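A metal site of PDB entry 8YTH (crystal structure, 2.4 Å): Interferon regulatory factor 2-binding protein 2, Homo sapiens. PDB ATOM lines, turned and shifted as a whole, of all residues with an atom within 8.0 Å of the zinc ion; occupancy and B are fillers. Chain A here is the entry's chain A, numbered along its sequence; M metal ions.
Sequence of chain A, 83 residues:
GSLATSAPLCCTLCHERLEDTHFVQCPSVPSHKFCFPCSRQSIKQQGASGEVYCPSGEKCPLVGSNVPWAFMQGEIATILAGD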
ATOM      1  N   CYS A  10      13.413  22.136  15.835  1.00  0.00           N
ATOM      2  CA  CYS A  10      13.346  20.692  15.671  1.00  0.00           C
ATOM      3  C   CYS A  10      13.837  20.352  14.278  1.00  0.00           C
ATOM      4  O   CYS A  10      13.937  21.208  13.400  1.00  0.00           O
ATOM      5  CB  CYS A  10      11.928  20.157  15.952  1.00  0.00           C
ATOM      6  SG  CYS A  10      10.852  19.785  14.588  1.00  0.00           S
ATOM      7  N   CYS A  11      14.199  19.083  14.109  1.00  0.00           N
ATOM      8  CA  CYS A  11      14.924  18.626  12.937  1.00  0.00           C
ATOM      9  C   CYS A  11      14.033  18.720  11.706  1.00  0.00           C
ATOM     10  O   CYS A  11      12.878  18.312  11.729  1.00  0.00           O
ATOM     11  CB  CYS A  11      15.400  17.195  13.154  1.00  0.00           C
ATOM     12  SG  CYS A  11      16.263  16.457  11.765  1.00  0.00           S
ATOM     13  N   THR A  12      14.567  19.289  10.616  1.00  0.00           N
ATOM     14  CA  THR A  12      13.700  19.451   9.458  1.00  0.00           C
ATOM     15  C   THR A  12      13.578  18.171   8.640  1.00  0.00           C
ATOM     16  O   THR A  12      12.972  18.182   7.564  1.00  0.00           O
ATOM     17  CB  THR A  12      14.186  20.609   8.592  1.00  0.00           C
ATOM     18  OG1 THR A  12      13.261  20.832   7.521  1.00  0.00           O
ATOM     19  CG2 THR A  12      15.552  20.312   8.005  1.00  0.00           C
ATOM     20  N   LEU A  13      14.159  17.077   9.133  1.00  0.00           N
ATOM     21  CA  LEU A  13      14.051  15.761   8.504  1.00  0.00           C
ATOM     22  C   LEU A  13      13.211  14.808   9.350  1.00  0.00           C
ATOM     23  O   LEU A  13      12.191  14.278   8.877  1.00  0.00           O
ATOM     24  CB  LEU A  13      15.434  15.168   8.260  1.00  0.00           C
ATOM     25  CG  LEU A  13      16.392  15.992   7.402  1.00  0.00           C
ATOM     26  CD1 LEU A  13      17.698  15.233   7.157  1.00  0.00           C
ATOM     27  CD2 LEU A  13      15.746  16.388   6.092  1.00  0.00           C
ATOM     28  N   CYS A  14      13.612  14.558  10.589  1.00  0.00           N
ATOM     29  CA  CYS A  14      12.886  13.630  11.454  1.00  0.00           C
ATOM     30  C   CYS A  14      11.921  14.344  12.399  1.00  0.00           C
ATOM     31  O   CYS A  14      11.053  13.681  12.982  1.00  0.00           O
ATOM     32  CB  CYS A  14      13.871  12.797  12.274  1.00  0.00           C
ATOM     33  SG  CYS A  14      14.492  13.620  13.754  1.00  0.00           S
ATOM     34  N   HIS A  15      12.055  15.663  12.550  1.00  0.00           N
ATOM     35  CA  HIS A  15      11.130  16.477  13.340  1.00  0.00           C
ATOM     36  C   HIS A  15      11.168  16.120  14.823  1.00  0.00           C
ATOM     37  O   HIS A  15      10.161  16.148  15.527  1.00  0.00           O
ATOM     38  CB  HIS A  15       9.707  16.405  12.783  1.00  0.00           C
ATOM     39  CG  HIS A  15       9.592  16.891  11.379  1.00  0.00           C
ATOM     40  ND1 HIS A  15       9.479  18.224  11.052  1.00  0.00           N
ATOM     41  CD2 HIS A  15       9.627  16.213  10.200  1.00  0.00           C
ATOM     42  CE1 HIS A  15       9.403  18.352   9.740  1.00  0.00           C
ATOM     43  NE2 HIS A  15       9.504  17.141   9.202  1.00  0.00           N
ATOM     44  N   GLU A  16      12.362  15.797  15.305  1.00  0.00           N
ATOM     45  CA  GLU A  16      12.604  15.638  16.728  1.00  0.00           C
ATOM     46  C   GLU A  16      13.010  16.984  17.312  1.00  0.00           C
ATOM     47  O   GLU A  16      13.756  17.742  16.678  1.00  0.00           O
ATOM     48  CB  GLU A  16      13.701  14.593  16.971  1.00  0.00           C
ATOM     49  CG  GLU A  16      14.742  14.994  17.983  1.00  0.00           C
ATOM     50  CD  GLU A  16      14.627  14.210  19.278  1.00  0.00           C
ATOM     51  OE1 GLU A  16      13.867  13.210  19.293  1.00  0.00           O
ATOM     52  OE2 GLU A  16      15.287  14.593  20.262  1.00  0.00           O
ATOM     53  N   ARG A  17      12.500  17.301  18.495  1.00  0.00           N
ATOM     54  CA  ARG A  17      12.814  18.586  19.116  1.00  0.00           C
ATOM     55  C   ARG A  17      14.296  18.654  19.456  1.00  0.00           C
ATOM     56  O   ARG A  17      14.963  17.647  19.692  1.00  0.00           O
ATOM     57  CB  ARG A  17      11.960  18.811  20.370  1.00  0.00           C
ATOM     58  CG  ARG A  17      10.446  18.784  20.127  1.00  0.00           C
ATOM     59  CD  ARG A  17      10.001  19.748  19.015  1.00  0.00           C
ATOM     60  NE  ARG A  17      10.452  21.122  19.229  1.00  0.00           N
ATOM     61  CZ  ARG A  17      10.008  22.174  18.555  1.00  0.00           C
ATOM     62  NH1 ARG A  17       9.074  22.047  17.628  1.00  0.00           N
ATOM     63  NH2 ARG A  17      10.521  23.377  18.809  1.00  0.00           N
ATOM     64  N   LEU A  18      14.830  19.881  19.437  1.00  0.00           N
ATOM     65  CA  LEU A  18      16.245  20.153  19.643  1.00  0.00           C
ATOM     66  C   LEU A  18      16.432  21.193  20.733  1.00  0.00           C
ATOM     67  O   LEU A  18      17.354  22.009  20.706  1.00  0.00           O
ATOM     68  CB  LEU A  18      16.890  20.640  18.333  1.00  0.00           C
ATOM     69  CG  LEU A  18      16.515  19.843  17.079  1.00  0.00           C
ATOM     70  CD1 LEU A  18      17.055  20.503  15.822  1.00  0.00           C
ATOM     71  CD2 LEU A  18      17.013  18.396  17.191  1.00  0.00           C
ATOM     72  N   LYS A  33      17.653  22.882  10.321  1.00  0.00           N
ATOM     73  CA  LYS A  33      18.190  22.268  11.525  1.00  0.00           C
ATOM     74  C   LYS A  33      18.097  20.752  11.425  1.00  0.00           C
ATOM     75  O   LYS A  33      17.125  20.214  10.888  1.00  0.00           O
ATOM     76  CB  LYS A  33      17.449  22.752  12.783  1.00  0.00           C
ATOM     77  CG  LYS A  33      17.762  24.196  13.125  1.00  0.00           C
ATOM     78  CD  LYS A  33      16.945  24.670  14.304  1.00  0.00           C
ATOM     79  CE  LYS A  33      16.360  26.027  14.003  1.00  0.00           C
ATOM     80  NZ  LYS A  33      17.413  26.977  13.548  1.00  0.00           N
ATOM     81  N   PHE A  34      19.131  20.065  11.930  1.00  0.00           N
ATOM     82  CA  PHE A  34      19.237  18.626  11.818  1.00  0.00           C
ATOM     83  C   PHE A  34      19.764  18.046  13.122  1.00  0.00           C
ATOM     84  O   PHE A  34      20.759  18.535  13.656  1.00  0.00           O
ATOM     85  CB  PHE A  34      20.174  18.217  10.670  1.00  0.00           C
ATOM     86  CG  PHE A  34      19.979  18.997   9.399  1.00  0.00           C
ATOM     87  CD1 PHE A  34      18.980  18.656   8.498  1.00  0.00           C
ATOM     88  CD2 PHE A  34      20.810  20.070   9.104  1.00  0.00           C
ATOM     89  CE1 PHE A  34      18.806  19.377   7.323  1.00  0.00           C
ATOM     90  CE2 PHE A  34      20.639  20.800   7.931  1.00  0.00           C
ATOM     91  CZ  PHE A  34      19.634  20.448   7.051  1.00  0.00           C
ATOM     92  N   CYS A  35      19.115  17.000  13.621  1.00  0.00           N
ATOM     93  CA  CYS A  35      19.639  16.310  14.786  1.00  0.00           C
ATOM     94  C   CYS A  35      20.916  15.574  14.419  1.00  0.00           C
ATOM     95  O   CYS A  35      21.253  15.371  13.245  1.00  0.00           O
ATOM     96  CB  CYS A  35      18.606  15.323  15.334  1.00  0.00           C
ATOM     97  SG  CYS A  35      18.147  14.026  14.174  1.00  0.00           S
ATOM     98  N   PHE A  36      21.659  15.160  15.440  1.00  0.00           N
ATOM     99  CA  PHE A  36      22.896  14.435  15.166  1.00  0.00           C
ATOM    100  C   PHE A  36      22.657  13.120  14.415  1.00  0.00           C
ATOM    101  O   PHE A  36      23.368  12.867  13.433  1.00  0.00           O
ATOM    102  CB  PHE A  36      23.684  14.230  16.457  1.00  0.00           C
ATOM    103  CG  PHE A  36      24.707  15.299  16.701  1.00  0.00           C
ATOM    104  CD1 PHE A  36      24.359  16.629  16.574  1.00  0.00           C
ATOM    105  CD2 PHE A  36      26.018  14.979  17.032  1.00  0.00           C
ATOM    106  CE1 PHE A  36      25.289  17.626  16.782  1.00  0.00           C
ATOM    107  CE2 PHE A  36      26.956  15.973  17.246  1.00  0.00           C
ATOM    108  CZ  PHE A  36      26.584  17.300  17.115  1.00  0.00           C
ATOM    109  N   PRO A  37      21.675  12.285  14.785  1.00  0.00           N
ATOM    110  CA  PRO A  37      21.412  11.091  13.955  1.00  0.00           C
ATOM    111  C   PRO A  37      21.161  11.394  12.497  1.00  0.00           C
ATOM    112  O   PRO A  37      21.746  10.735  11.629  1.00  0.00           O
ATOM    113  CB  PRO A  37      20.188  10.472  14.646  1.00  0.00           C
ATOM    114  CG  PRO A  37      20.360  10.828  16.061  1.00  0.00           C
ATOM    115  CD  PRO A  37      20.902  12.243  16.040  1.00  0.00           C
ATOM    116  N   CYS A  38      20.325  12.398  12.188  1.00  0.00           N
ATOM    117  CA  CYS A  38      20.079  12.734  10.792  1.00  0.00           C
ATOM    118  C   CYS A  38      21.338  13.258  10.111  1.00  0.00           C
ATOM    119  O   CYS A  38      21.581  12.969   8.929  1.00  0.00           O
ATOM    120  CB  CYS A  38      18.938  13.756  10.681  1.00  0.00           C
ATOM    121  SG  CYS A  38      17.243  13.091  10.811  1.00  0.00           S
ATOM    122  N   SER A  39      22.155  14.032  10.832  1.00  0.00           N
ATOM    123  CA  SER A  39      23.427  14.466  10.259  1.00  0.00           C
ATOM    124  C   SER A  39      24.362  13.294  10.012  1.00  0.00           C
ATOM    125  O   SER A  39      25.066  13.267   9.000  1.00  0.00           O
ATOM    126  CB  SER A  39      24.097  15.494  11.180  1.00  0.00           C
ATOM    127  OG  SER A  39      23.246  16.599  11.420  1.00  0.00           O
HETATM  128 ZN    ZN M   1      16.435  14.269  12.627  1.00  0.00          ZN
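The backbone carbonyl oxygen of Cys 35 sits at hydrogen-bond distance from the side-chain hydroxyl of Ser 39 (3.0 Å). The side-chain sulfur of Cys 14 sits close to the backbone NH of Glu 16 (3.4 Å). The backbone NH of Leu 13 sits close to the side-chain sulfur of Cys 11 (3.4 Å). A ring nitrogen (ND1) of His 15 lies close to the backbone carbonyl oxygen (O) of Cys 11 (3.5 Å). The backbone NH of Cys 11 sits at hydrogen-bond distance from the backbone carbonyl oxygen of Glu 16, at 2.9 Å.
Of the 16 residues printed, 4 come within 4 Å of the zinc ion.
The side-chain sulfur (SG) of Cys 38 is bound to the zinc ion (2.3 Å). SG of Cys 35 binds the zinc ion (2.3 Å). The side-chain sulfur (SG) of Cys 14 binds the zinc ion (2.3 Å). The zinc ion is bound by SG of Cys 11, at 2.4 Å.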
